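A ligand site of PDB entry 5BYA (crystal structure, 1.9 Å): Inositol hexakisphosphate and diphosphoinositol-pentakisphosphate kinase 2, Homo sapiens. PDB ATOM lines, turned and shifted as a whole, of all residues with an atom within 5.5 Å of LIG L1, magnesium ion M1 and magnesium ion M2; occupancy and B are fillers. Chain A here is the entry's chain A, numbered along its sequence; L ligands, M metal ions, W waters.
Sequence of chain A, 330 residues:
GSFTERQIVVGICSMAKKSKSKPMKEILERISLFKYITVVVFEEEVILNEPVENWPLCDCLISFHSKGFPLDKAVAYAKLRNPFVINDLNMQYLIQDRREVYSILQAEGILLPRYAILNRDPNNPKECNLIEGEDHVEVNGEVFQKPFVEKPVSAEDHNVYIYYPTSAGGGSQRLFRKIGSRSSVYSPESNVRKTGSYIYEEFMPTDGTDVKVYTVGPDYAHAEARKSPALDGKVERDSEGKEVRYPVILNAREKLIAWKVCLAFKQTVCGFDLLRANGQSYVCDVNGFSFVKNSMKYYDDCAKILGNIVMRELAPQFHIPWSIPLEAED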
ATOM      1  N   ARG A  98     -33.984   1.309  33.466  1.00  0.00           N
ATOM      2  CA  ARG A  98     -34.214   1.294  32.008  1.00  0.00           C
ATOM      3  C   ARG A  98     -35.628   1.726  31.619  1.00  0.00           C
ATOM      4  O   ARG A  98     -35.838   2.321  30.548  1.00  0.00           O
ATOM      5  CB  ARG A  98     -33.916  -0.089  31.402  1.00  0.00           C
ATOM      6  CG  ARG A  98     -32.481  -0.572  31.555  1.00  0.00           C
ATOM      7  CD  ARG A  98     -32.225  -1.826  30.699  1.00  0.00           C
ATOM      8  NE  ARG A  98     -31.001  -2.520  31.126  1.00  0.00           N
ATOM      9  CZ  ARG A  98     -29.782  -2.212  30.693  1.00  0.00           C
ATOM     10  NH1 ARG A  98     -29.625  -1.242  29.797  1.00  0.00           N
ATOM     11  NH2 ARG A  98     -28.712  -2.862  31.147  1.00  0.00           N
ATOM     12  N   TYR A 102     -36.277   4.820  28.970  1.00  0.00           N
ATOM     13  CA  TYR A 102     -37.101   4.681  27.762  1.00  0.00           C
ATOM     14  C   TYR A 102     -38.275   5.650  27.731  1.00  0.00           C
ATOM     15  O   TYR A 102     -38.656   6.158  26.668  1.00  0.00           O
ATOM     16  CB  TYR A 102     -37.593   3.236  27.609  1.00  0.00           C
ATOM     17  CG  TYR A 102     -36.598   2.340  26.890  1.00  0.00           C
ATOM     18  CD1 TYR A 102     -35.241   2.668  26.830  1.00  0.00           C
ATOM     19  CD2 TYR A 102     -37.022   1.176  26.271  1.00  0.00           C
ATOM     20  CE1 TYR A 102     -34.333   1.858  26.164  1.00  0.00           C
ATOM     21  CE2 TYR A 102     -36.131   0.351  25.615  1.00  0.00           C
ATOM     22  CZ  TYR A 102     -34.792   0.695  25.560  1.00  0.00           C
ATOM     23  OH  TYR A 102     -33.919  -0.138  24.901  1.00  0.00           O
ATOM     24  N   PRO A 113     -36.165   1.277  20.049  1.00  0.00           N
ATOM     25  CA  PRO A 113     -36.854   0.046  19.656  1.00  0.00           C
ATOM     26  C   PRO A 113     -38.279  -0.021  20.213  1.00  0.00           C
ATOM     27  O   PRO A 113     -38.519   0.451  21.327  1.00  0.00           O
ATOM     28  CB  PRO A 113     -36.005  -1.055  20.299  1.00  0.00           C
ATOM     29  CG  PRO A 113     -34.656  -0.433  20.518  1.00  0.00           C
ATOM     30  CD  PRO A 113     -34.934   1.004  20.812  1.00  0.00           C
ATOM     31  N   VAL A 149     -35.166  -8.832  22.217  1.00  0.00           N
ATOM     32  CA  VAL A 149     -34.186  -8.537  23.249  1.00  0.00           C
ATOM     33  C   VAL A 149     -34.880  -8.419  24.610  1.00  0.00           C
ATOM     34  O   VAL A 149     -35.993  -7.879  24.717  1.00  0.00           O
ATOM     35  CB  VAL A 149     -33.375  -7.252  22.920  1.00  0.00           C
ATOM     36  CG1 VAL A 149     -32.270  -6.996  23.950  1.00  0.00           C
ATOM     37  CG2 VAL A 149     -32.752  -7.348  21.533  1.00  0.00           C
ATOM     38  N   LYS A 151     -34.090  -7.161  28.478  1.00  0.00           N
ATOM     39  CA  LYS A 151     -33.192  -6.406  29.352  1.00  0.00           C
ATOM     40  C   LYS A 151     -33.714  -6.329  30.772  1.00  0.00           C
ATOM     41  O   LYS A 151     -34.881  -6.008  30.979  1.00  0.00           O
ATOM     42  CB  LYS A 151     -32.989  -4.984  28.817  1.00  0.00           C
ATOM     43  CG  LYS A 151     -32.597  -4.921  27.365  1.00  0.00           C
ATOM     44  CD  LYS A 151     -32.201  -3.507  26.960  1.00  0.00           C
ATOM     45  CE  LYS A 151     -31.863  -3.468  25.490  1.00  0.00           C
ATOM     46  NZ  LYS A 151     -31.560  -2.078  25.039  1.00  0.00           N
ATOM     47  N   ALA A 155     -30.599  -0.774  35.072  1.00  0.00           N
ATOM     48  CA  ALA A 155     -29.608  -0.386  34.072  1.00  0.00           C
ATOM     49  C   ALA A 155     -28.188  -0.822  34.431  1.00  0.00           C
ATOM     50  O   ALA A 155     -27.313  -0.879  33.559  1.00  0.00           O
ATOM     51  CB  ALA A 155     -29.646   1.123  33.838  1.00  0.00           C
ATOM     52  N   ASP A 157     -27.601  -3.791  35.564  1.00  0.00           N
ATOM     53  CA  ASP A 157     -27.566  -5.223  35.274  1.00  0.00           C
ATOM     54  C   ASP A 157     -27.389  -5.417  33.773  1.00  0.00           C
ATOM     55  O   ASP A 157     -28.308  -5.156  32.999  1.00  0.00           O
ATOM     56  CB  ASP A 157     -28.854  -5.892  35.782  1.00  0.00           C
ATOM     57  CG  ASP A 157     -28.837  -7.409  35.643  1.00  0.00           C
ATOM     58  OD1 ASP A 157     -28.030  -7.965  34.864  1.00  0.00           O
ATOM     59  OD2 ASP A 157     -29.644  -8.062  36.333  1.00  0.00           O
ATOM     60  N   HIS A 158     -26.201  -5.857  33.370  1.00  0.00           N
ATOM     61  CA  HIS A 158     -25.840  -5.994  31.958  1.00  0.00           C
ATOM     62  C   HIS A 158     -26.132  -7.384  31.374  1.00  0.00           C
ATOM     63  O   HIS A 158     -25.706  -7.704  30.276  1.00  0.00           O
ATOM     64  CB  HIS A 158     -24.371  -5.599  31.747  1.00  0.00           C
ATOM     65  CG  HIS A 158     -24.060  -4.229  32.255  1.00  0.00           C
ATOM     66  ND1 HIS A 158     -24.495  -3.083  31.633  1.00  0.00           N
ATOM     67  CD2 HIS A 158     -23.401  -3.821  33.375  1.00  0.00           C
ATOM     68  CE1 HIS A 158     -24.110  -2.030  32.320  1.00  0.00           C
ATOM     69  NE2 HIS A 158     -23.448  -2.451  33.384  1.00  0.00           N
ATOM     70  N   VAL A 160     -28.171  -8.858  29.461  1.00  0.00           N
ATOM     71  CA  VAL A 160     -29.129  -8.664  28.380  1.00  0.00           C
ATOM     72  C   VAL A 160     -29.121  -9.919  27.508  1.00  0.00           C
ATOM     73  O   VAL A 160     -28.048 -10.395  27.098  1.00  0.00           O
ATOM     74  CB  VAL A 160     -28.751  -7.409  27.551  1.00  0.00           C
ATOM     75  CG1 VAL A 160     -29.554  -7.314  26.277  1.00  0.00           C
ATOM     76  CG2 VAL A 160     -28.925  -6.138  28.390  1.00  0.00           C
ATOM     77  N   ILE A 162     -30.599 -12.055  24.074  1.00  0.00           N
ATOM     78  CA  ILE A 162     -31.229 -12.021  22.758  1.00  0.00           C
ATOM     79  C   ILE A 162     -31.756 -13.421  22.408  1.00  0.00           C
ATOM     80  O   ILE A 162     -31.057 -14.408  22.608  1.00  0.00           O
ATOM     81  CB  ILE A 162     -30.231 -11.524  21.694  1.00  0.00           C
ATOM     82  CG1 ILE A 162     -29.749 -10.109  22.096  1.00  0.00           C
ATOM     83  CG2 ILE A 162     -30.866 -11.560  20.315  1.00  0.00           C
ATOM     84  CD1 ILE A 162     -28.749  -9.482  21.180  1.00  0.00           C
ATOM     85  N   LEU A 175     -25.591 -11.833  26.995  1.00  0.00           N
ATOM     86  CA  LEU A 175     -24.556 -10.818  27.113  1.00  0.00           C
ATOM     87  C   LEU A 175     -24.236 -10.579  28.590  1.00  0.00           C
ATOM     88  O   LEU A 175     -25.059 -10.853  29.453  1.00  0.00           O
ATOM     89  CB  LEU A 175     -25.006  -9.513  26.447  1.00  0.00           C
ATOM     90  CG  LEU A 175     -25.087  -9.442  24.913  1.00  0.00           C
ATOM     91  CD1 LEU A 175     -26.007 -10.491  24.298  1.00  0.00           C
ATOM     92  CD2 LEU A 175     -25.555  -8.055  24.521  1.00  0.00           C
ATOM     93  N   GLU A 201     -37.977  -6.000  23.786  1.00  0.00           N
ATOM     94  CA  GLU A 201     -37.942  -5.081  22.657  1.00  0.00           C
ATOM     95  C   GLU A 201     -37.562  -5.746  21.349  1.00  0.00           C
ATOM     96  O   GLU A 201     -36.921  -6.811  21.332  1.00  0.00           O
ATOM     97  CB  GLU A 201     -37.033  -3.871  22.952  1.00  0.00           C
ATOM     98  CG  GLU A 201     -35.558  -4.180  23.079  1.00  0.00           C
ATOM     99  CD  GLU A 201     -34.760  -2.989  23.601  1.00  0.00           C
ATOM    100  OE1 GLU A 201     -33.838  -2.565  22.911  1.00  0.00           O
ATOM    101  OE2 GLU A 201     -35.057  -2.485  24.710  1.00  0.00           O
ATOM    102  N   GLU A 202     -37.974  -5.126  20.245  1.00  0.00           N
ATOM    103  CA  GLU A 202     -37.667  -5.630  18.902  1.00  0.00           C
ATOM    104  C   GLU A 202     -36.169  -5.513  18.609  1.00  0.00           C
ATOM    105  O   GLU A 202     -35.543  -4.496  18.925  1.00  0.00           O
ATOM    106  CB  GLU A 202     -38.481  -4.872  17.847  1.00  0.00           C
ATOM    107  CG  GLU A 202     -37.927  -3.500  17.529  1.00  0.00           C
ATOM    108  CD  GLU A 202     -38.845  -2.657  16.659  1.00  0.00           C
ATOM    109  OE1 GLU A 202     -39.804  -3.203  16.074  1.00  0.00           O
ATOM    110  OE2 GLU A 202     -38.613  -1.427  16.575  1.00  0.00           O
ATOM    111  N   PHE A 203     -35.606  -6.570  18.032  1.00  0.00           N
ATOM    112  CA  PHE A 203     -34.197  -6.627  17.642  1.00  0.00           C
ATOM    113  C   PHE A 203     -34.007  -5.757  16.406  1.00  0.00           C
ATOM    114  O   PHE A 203     -34.675  -5.940  15.388  1.00  0.00           O
ATOM    115  CB  PHE A 203     -33.776  -8.072  17.356  1.00  0.00           C
ATOM    116  CG  PHE A 203     -32.329  -8.222  16.975  1.00  0.00           C
ATOM    117  CD1 PHE A 203     -31.342  -8.349  17.960  1.00  0.00           C
ATOM    118  CD2 PHE A 203     -31.939  -8.246  15.636  1.00  0.00           C
ATOM    119  CE1 PHE A 203     -30.002  -8.490  17.609  1.00  0.00           C
ATOM    120  CE2 PHE A 203     -30.602  -8.378  15.283  1.00  0.00           C
ATOM    121  CZ  PHE A 203     -29.629  -8.498  16.275  1.00  0.00           C
ATOM    122  N   MET A 204     -33.087  -4.801  16.509  1.00  0.00           N
ATOM    123  CA  MET A 204     -32.785  -3.920  15.386  1.00  0.00           C
ATOM    124  C   MET A 204     -31.554  -4.463  14.665  1.00  0.00           C
ATOM    125  O   MET A 204     -30.487  -4.580  15.275  1.00  0.00           O
ATOM    126  CB  MET A 204     -32.521  -2.484  15.876  1.00  0.00           C
ATOM    127  CG  MET A 204     -33.515  -1.959  16.911  1.00  0.00           C
ATOM    128  SD  MET A 204     -35.256  -1.986  16.396  1.00  0.00           S
ATOM    129  CE  MET A 204     -35.195  -0.987  14.914  1.00  0.00           C
ATOM    130  N   PRO A 205     -31.706  -4.797  13.366  1.00  0.00           N
ATOM    131  CA  PRO A 205     -30.599  -5.373  12.615  1.00  0.00           C
ATOM    132  C   PRO A 205     -29.591  -4.295  12.186  1.00  0.00           C
ATOM    133  O   PRO A 205     -29.918  -3.427  11.385  1.00  0.00           O
ATOM    134  CB  PRO A 205     -31.284  -6.005  11.407  1.00  0.00           C
ATOM    135  CG  PRO A 205     -32.515  -5.181  11.198  1.00  0.00           C
ATOM    136  CD  PRO A 205     -32.922  -4.649  12.549  1.00  0.00           C
ATOM    137  N   ASP A 210     -22.222  -1.589  17.177  1.00  0.00           N
ATOM    138  CA  ASP A 210     -22.938  -0.564  17.944  1.00  0.00           C
ATOM    139  C   ASP A 210     -22.201   0.750  17.740  1.00  0.00           C
ATOM    140  O   ASP A 210     -20.974   0.763  17.665  1.00  0.00           O
ATOM    141  CB  ASP A 210     -22.862  -0.851  19.443  1.00  0.00           C
ATOM    142  CG  ASP A 210     -23.374  -2.209  19.808  1.00  0.00           C
ATOM    143  OD1 ASP A 210     -24.264  -2.727  19.120  1.00  0.00           O
ATOM    144  OD2 ASP A 210     -22.881  -2.760  20.826  1.00  0.00           O
ATOM    145  N   SER A 228     -20.776  -5.604  17.923  1.00  0.00           N
ATOM    146  CA  SER A 228     -21.877  -5.886  18.847  1.00  0.00           C
ATOM    147  C   SER A 228     -21.571  -7.153  19.655  1.00  0.00           C
ATOM    148  O   SER A 228     -21.251  -8.174  19.068  1.00  0.00           O
ATOM    149  CB  SER A 228     -23.193  -6.069  18.095  1.00  0.00           C
ATOM    150  OG  SER A 228     -24.205  -6.554  18.980  1.00  0.00           O
ATOM    151  N   PRO A 229     -21.676  -7.083  21.001  1.00  0.00           N
ATOM    152  CA  PRO A 229     -21.453  -8.266  21.844  1.00  0.00           C
ATOM    153  C   PRO A 229     -22.355  -9.429  21.442  1.00  0.00           C
ATOM    154  O   PRO A 229     -22.007 -10.596  21.639  1.00  0.00           O
ATOM    155  CB  PRO A 229     -21.834  -7.789  23.248  1.00  0.00           C
ATOM    156  CG  PRO A 229     -21.674  -6.317  23.201  1.00  0.00           C
ATOM    157  CD  PRO A 229     -22.008  -5.892  21.799  1.00  0.00           C
ATOM    158  N   ALA A 230     -23.506  -9.090  20.849  1.00  0.00           N
ATOM    159  CA  ALA A 230     -24.527 -10.047  20.449  1.00  0.00           C
ATOM    160  C   ALA A 230     -24.172 -10.921  19.235  1.00  0.00           C
ATOM    161  O   ALA A 230     -24.886 -11.890  18.947  1.00  0.00           O
ATOM    162  CB  ALA A 230     -25.824  -9.313  20.198  1.00  0.00           C
ATOM    163  N   ASP A 273     -25.932   4.692  23.505  1.00  0.00           N
ATOM    164  CA  ASP A 273     -25.728   3.788  22.378  1.00  0.00           C
ATOM    165  C   ASP A 273     -26.744   4.046  21.288  1.00  0.00           C
ATOM    166  O   ASP A 273     -27.921   4.284  21.586  1.00  0.00           O
ATOM    167  CB  ASP A 273     -25.846   2.325  22.812  1.00  0.00           C
ATOM    168  CG  ASP A 273     -24.807   1.931  23.831  1.00  0.00           C
ATOM    169  OD1 ASP A 273     -23.682   2.468  23.792  1.00  0.00           O
ATOM    170  OD2 ASP A 273     -25.103   1.057  24.658  1.00  0.00           O
ATOM    171  N   LEU A 275     -28.184   2.365  17.545  1.00  0.00           N
ATOM    172  CA  LEU A 275     -28.234   1.241  16.624  1.00  0.00           C
ATOM    173  C   LEU A 275     -28.608   1.802  15.269  1.00  0.00           C
ATOM    174  O   LEU A 275     -29.705   2.345  15.091  1.00  0.00           O
ATOM    175  CB  LEU A 275     -29.262   0.196  17.097  1.00  0.00           C
ATOM    176  CG  LEU A 275     -29.078  -0.326  18.524  1.00  0.00           C
ATOM    177  CD1 LEU A 275     -30.221  -1.288  18.871  1.00  0.00           C
ATOM    178  CD2 LEU A 275     -27.720  -1.004  18.718  1.00  0.00           C
ATOM    179  N   CYS A 284     -30.710   2.834  22.349  1.00  0.00           N
ATOM    180  CA  CYS A 284     -31.093   1.623  23.079  1.00  0.00           C
ATOM    181  C   CYS A 284     -30.602   1.617  24.528  1.00  0.00           C
ATOM    182  O   CYS A 284     -30.907   0.682  25.289  1.00  0.00           O
ATOM    183  CB  CYS A 284     -30.597   0.363  22.331  1.00  0.00           C
ATOM    184  SG  CYS A 284     -28.815   0.060  22.434  1.00  0.00           S
ATOM    185  N   ASP A 285     -29.881   2.666  24.931  1.00  0.00           N
ATOM    186  CA  ASP A 285     -29.200   2.695  26.238  1.00  0.00           C
ATOM    187  C   ASP A 285     -28.694   4.113  26.448  1.00  0.00           C
ATOM    188  O   ASP A 285     -28.041   4.669  25.577  1.00  0.00           O
ATOM    189  CB  ASP A 285     -28.028   1.700  26.201  1.00  0.00           C
ATOM    190  CG  ASP A 285     -27.371   1.480  27.566  1.00  0.00           C
ATOM    191  OD1 ASP A 285     -27.988   1.696  28.621  1.00  0.00           O
ATOM    192  OD2 ASP A 285     -26.207   1.039  27.579  1.00  0.00           O
ATOM    193  N   VAL A 286     -28.986   4.695  27.610  1.00  0.00           N
ATOM    194  CA  VAL A 286     -28.426   5.998  28.010  1.00  0.00           C
ATOM    195  C   VAL A 286     -27.741   5.796  29.358  1.00  0.00           C
ATOM    196  O   VAL A 286     -28.403   5.505  30.367  1.00  0.00           O
ATOM    197  CB  VAL A 286     -29.513   7.106  28.121  1.00  0.00           C
ATOM    198  CG1 VAL A 286     -28.895   8.447  28.547  1.00  0.00           C
ATOM    199  CG2 VAL A 286     -30.269   7.263  26.796  1.00  0.00           C
ATOM    200  N   ASN A 287     -26.423   5.928  29.378  1.00  0.00           N
ATOM    201  CA  ASN A 287     -25.637   5.589  30.557  1.00  0.00           C
ATOM    202  C   ASN A 287     -25.312   6.764  31.473  1.00  0.00           C
ATOM    203  O   ASN A 287     -24.966   6.569  32.642  1.00  0.00           O
ATOM    204  CB  ASN A 287     -24.357   4.854  30.138  1.00  0.00           C
ATOM    205  CG  ASN A 287     -24.665   3.543  29.438  1.00  0.00           C
ATOM    206  OD1 ASN A 287     -25.474   2.752  29.930  1.00  0.00           O
ATOM    207  ND2 ASN A 287     -24.035   3.302  28.287  1.00  0.00           N
HETATM  208  P1  LIG L   1     -26.137  -2.152  28.612  1.00  0.00           P
HETATM  209  O1  LIG L   1     -26.795  -1.086  29.466  1.00  0.00           O
HETATM  210  O2  LIG L   1     -25.859  -3.415  29.383  1.00  0.00           O
HETATM  211  O3  LIG L   1     -25.011  -1.637  27.765  1.00  0.00           O
HETATM  212  P2  LIG L   1     -27.706  -2.145  26.114  1.00  0.00           P
HETATM  213  O4  LIG L   1     -29.161  -1.750  26.051  1.00  0.00           O
HETATM  214  O5  LIG L   1     -26.662  -1.212  25.546  1.00  0.00           O
HETATM  215  O6  LIG L   1     -27.352  -2.605  27.627  1.00  0.00           O
HETATM  216  O7  LIG L   1     -27.592  -3.556  25.344  1.00  0.00           O
HETATM  217  C1  LIG L   1     -26.322  -4.212  25.231  1.00  0.00           C
HETATM  218  C2  LIG L   1     -26.020  -4.534  23.770  1.00  0.00           C
HETATM  219  O8  LIG L   1     -27.042  -5.389  23.234  1.00  0.00           O
HETATM  220  C3  LIG L   1     -26.016  -3.322  22.854  1.00  0.00           C
HETATM  221  O9  LIG L   1     -24.733  -2.691  22.813  1.00  0.00           O
HETATM  222  C4  LIG L   1     -26.399  -3.897  21.511  1.00  0.00           C
HETATM  223  O10 LIG L   1     -25.272  -4.507  20.872  1.00  0.00           O
HETATM  224  C5  LIG L   1     -27.340  -5.015  21.886  1.00  0.00           C
HETATM  225  N1  LIG L   1     -28.752  -4.538  21.821  1.00  0.00           N
HETATM  226  C6  LIG L   1     -29.432  -3.942  22.825  1.00  0.00           C
HETATM  227  N2  LIG L   1     -30.693  -3.646  22.443  1.00  0.00           N
HETATM  228  C7  LIG L   1     -30.825  -4.058  21.157  1.00  0.00           C
HETATM  229  C8  LIG L   1     -31.921  -4.055  20.146  1.00  0.00           C
HETATM  230  N3  LIG L   1     -33.135  -3.540  20.432  1.00  0.00           N
HETATM  231  N4  LIG L   1     -31.644  -4.580  18.923  1.00  0.00           N
HETATM  232  C9  LIG L   1     -30.448  -5.096  18.613  1.00  0.00           C
HETATM  233  N5  LIG L   1     -29.425  -5.143  19.492  1.00  0.00           N
HETATM  234  C10 LIG L   1     -29.545  -4.639  20.748  1.00  0.00           C
HETATM  235  C1  LG2 L   2     -18.606   0.519  30.713  1.00  0.00           C
HETATM  236  C2  LG2 L   2     -18.440   1.354  31.981  1.00  0.00           C
HETATM  237  C3  LG2 L   2     -17.964   0.351  33.064  1.00  0.00           C
HETATM  238  C4  LG2 L   2     -16.564  -0.201  32.726  1.00  0.00           C
HETATM  239  C5  LG2 L   2     -16.517  -0.789  31.303  1.00  0.00           C
HETATM  240  C6  LG2 L   2     -17.239   0.043  30.225  1.00  0.00           C
HETATM  241  O1  LG2 L   2     -11.790  -2.452  29.262  1.00  0.00           O
HETATM  242  P1  LG2 L   2     -11.721  -3.281  30.471  1.00  0.00           P
HETATM  243  O2  LG2 L   2     -12.307  -4.641  30.432  1.00  0.00           O
HETATM  244  O3  LG2 L   2     -10.627  -3.000  31.434  1.00  0.00           O
HETATM  245  C7  LG2 L   2     -13.078  -2.510  31.425  1.00  0.00           C
HETATM  246  P2  LG2 L   2     -14.596  -2.387  30.420  1.00  0.00           P
HETATM  247  O4  LG2 L   2     -15.553  -3.450  30.826  1.00  0.00           O
HETATM  248  O5  LG2 L   2     -14.237  -2.254  28.994  1.00  0.00           O
HETATM  249  O6  LG2 L   2     -15.154  -0.949  30.927  1.00  0.00           O
HETATM  250  O7  LG2 L   2     -17.420  -0.796  29.078  1.00  0.00           O
HETATM  251  P3  LG2 L   2     -17.243  -0.350  27.556  1.00  0.00           P
HETATM  252  O8  LG2 L   2     -18.541  -0.788  26.964  1.00  0.00           O
HETATM  253  O9  LG2 L   2     -16.980   1.094  27.552  1.00  0.00           O
HETATM  254  O10 LG2 L   2     -16.088  -1.178  27.135  1.00  0.00           O
HETATM  255  O11 LG2 L   2     -16.251  -1.264  33.663  1.00  0.00           O
HETATM  256  P4  LG2 L   2     -15.144  -1.134  34.823  1.00  0.00           P
HETATM  257  O12 LG2 L   2     -15.894  -0.662  35.993  1.00  0.00           O
HETATM  258  O13 LG2 L   2     -14.592  -2.494  34.920  1.00  0.00           O
HETATM  259  O14 LG2 L   2     -14.180  -0.143  34.263  1.00  0.00           O
HETATM  260  O15 LG2 L   2     -17.976   0.942  34.381  1.00  0.00           O
HETATM  261  P5  LG2 L   2     -19.090   0.463  35.431  1.00  0.00           P
HETATM  262  O16 LG2 L   2     -19.045   1.473  36.499  1.00  0.00           O
HETATM  263  O17 LG2 L   2     -20.331   0.431  34.633  1.00  0.00           O
HETATM  264  O18 LG2 L   2     -18.577  -0.874  35.825  1.00  0.00           O
HETATM  265  O19 LG2 L   2     -17.441   2.402  31.790  1.00  0.00           O
HETATM  266  P6  LG2 L   2     -17.723   3.974  31.953  1.00  0.00           P
HETATM  267  O20 LG2 L   2     -18.458   4.081  33.235  1.00  0.00           O
HETATM  268  O21 LG2 L   2     -16.379   4.562  31.908  1.00  0.00           O
HETATM  269  O22 LG2 L   2     -18.552   4.291  30.747  1.00  0.00           O
HETATM  270  O23 LG2 L   2     -19.296   1.232  29.688  1.00  0.00           O
HETATM  271  P7  LG2 L   2     -20.777   0.788  29.257  1.00  0.00           P
HETATM  272  O24 LG2 L   2     -20.805  -0.661  28.998  1.00  0.00           O
HETATM  273  O25 LG2 L   2     -21.737   1.387  30.217  1.00  0.00           O
HETATM  274  C8  LG2 L   2     -20.917   1.683  27.646  1.00  0.00           C
HETATM  275  P8  LG2 L   2     -21.940   0.806  26.466  1.00  0.00           P
HETATM  276  O26 LG2 L   2     -21.318  -0.501  26.210  1.00  0.00           O
HETATM  277  O27 LG2 L   2     -21.936   1.729  25.310  1.00  0.00           O
HETATM  278  O28 LG2 L   2     -23.241   0.708  27.174  1.00  0.00           O
HETATM  279 MG    MG M   1     -26.168   0.790  29.713  1.00  0.00          MG
HETATM  280 MG    MG M   2     -24.969  -0.245  26.268  1.00  0.00          MG
HETATM  281 MG    MG M   3     -20.633  -1.853  27.379  1.00  0.00          MG
HETATM  282  O   HOH W   1     -22.486  -2.820  27.817  1.00  0.00           O
HETATM  283  O   HOH W   2     -26.686   0.944  31.667  1.00  0.00           O
HETATM  284  O   HOH W   3     -24.142   0.215  29.898  1.00  0.00           O
HETATM  285  O   HOH W   4     -23.821  -1.487  25.007  1.00  0.00           O
HETATM  286  O   HOH W   5     -25.317  -5.678  28.230  1.00  0.00           O
HETATM  287  O   HOH W   6     -27.081  -5.835  17.957  1.00  0.00           O
HETATM  288  O   HOH W   7     -21.534  -2.244  23.367  1.00  0.00           O
HETATM  289  O   HOH W   8     -31.215  -0.032  27.940  1.00  0.00           O
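An oxygen (O4) of LIG L1 lies within salt-bridge range of the side-chain amino group of Lys 151, at 2.6 Å. A ring nitrogen (ND1) of His 158 sits at hydrogen-bond distance from an oxygen (O2) of LIG L1, 2.7 Å away. The side-chain carboxylate (OD1) of Asp 210 lies within hydrogen-bond range of an oxygen (O10) of LIG L1, 2.7 Å away. The side-chain carboxylate (OE1) of Glu 201 lies within hydrogen-bond range of a nitrogen (N3) of LIG L1. The backbone NH (N) of Met 204 lies within hydrogen-bond range of a nitrogen (N4) of LIG L1. NH2 of Arg 98 lies within salt-bridge range of O2 of LIG L1 (3.4 Å). The side-chain hydroxyl of Ser 228 lies within hydrogen-bond range of an oxygen (O10) of LIG L1 (3.0 Å). N3 of LIG L1 is in hydrogen-bond range of O of Glu 202. The backbone carbonyl oxygen (O) of Cys 284 lies close to an oxygen (O4) of LIG L1, 3.1 Å away. The side-chain amide nitrogen (ND2) of Asn 287 sits close to an oxygen (O28) of LG2 L2, 2.9 Å away.
The backbone carbonyl oxygen of Asp 273 sits at hydrogen-bond distance from the backbone NH of Cys 284 (3.2 Å). The side-chain amino group (NZ) of Lys 151 lies within salt-bridge range of the side-chain carboxylate (OE1) of Glu 201, at 3.2 Å. The side-chain amino group (NZ) of Lys 151 is in hydrogen-bond range of the backbone carbonyl oxygen (O) of Cys 284 (2.8 Å). NZ of Lys 151 lies within hydrogen-bond range of OH of Tyr 102. The backbone carbonyl oxygen (O) of Glu 201 is in hydrogen-bond range of the backbone NH (N) of Val 149 (2.8 Å). OE2 of Glu 201 lies within hydrogen-bond range of OH of Tyr 102 (2.6 Å). NH2 of Arg 98 is in hydrogen-bond range of O of Asp 157 (3.0 Å). OH of Tyr 102 is in hydrogen-bond range of O of Cys 284, 3.1 Å away.
Pro 113 touches LIG L1. Val 149 touches LIG L1. CG2 of Val 160 touches O6 of LIG L1, at 3.9 Å. Leu 175 touches LIG L1. CD1 of Phe 203 touches C9 of LIG L1 (3.4 Å). Pro 229 touches LIG L1. Leu 275 touches LIG L1.
Within 4 Å of magnesium ion M1: Asp 285 and Asn 287.
Two residues have an atom within 4 Å of magnesium ion M2: Asp 273 and Asp 285. Along chain A the residues within 4 Å of magnesium ion M2 span positions 273 to 285.
Magnesium ion M1 is bound by O1 of LIG L1, water W2, OD1 of Asn 287, water W3, OD2 of Asp 285 and OD1 of Asp 285. Magnesium ion M1 has six donor atoms within binding distance.
Magnesium ion M2 is bound by an oxygen (O3) of LIG L1, the side-chain carboxylate (OD2) of Asp 273, an oxygen (O5) of LIG L1, water W4, an oxygen (O28) of LG2 L2 and the side-chain carboxylate (OD2) of Asp 285.
Water W3 bridges O25 of LG2 L2 (2.7 Å) and ND2 of Asn 287 (3.5 Å). Water W5 bridges O2 of LIG L1 (2.6 Å) and O of His 158 (2.9 Å). Water W6 bridges a nitrogen (N5) of LIG L1 (2.9 Å) and the side-chain hydroxyl of Ser 228 (3.1 Å). Water W8 lies within hydrogen-bond range of NH1 of Arg 98 (2.7 Å), O of Cys 284 (2.8 Å) and O4 of LIG L1 (3.3 Å). Water W7 lies within hydrogen-bond range of OD2 of Asp 210 and O9 of LIG L1.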
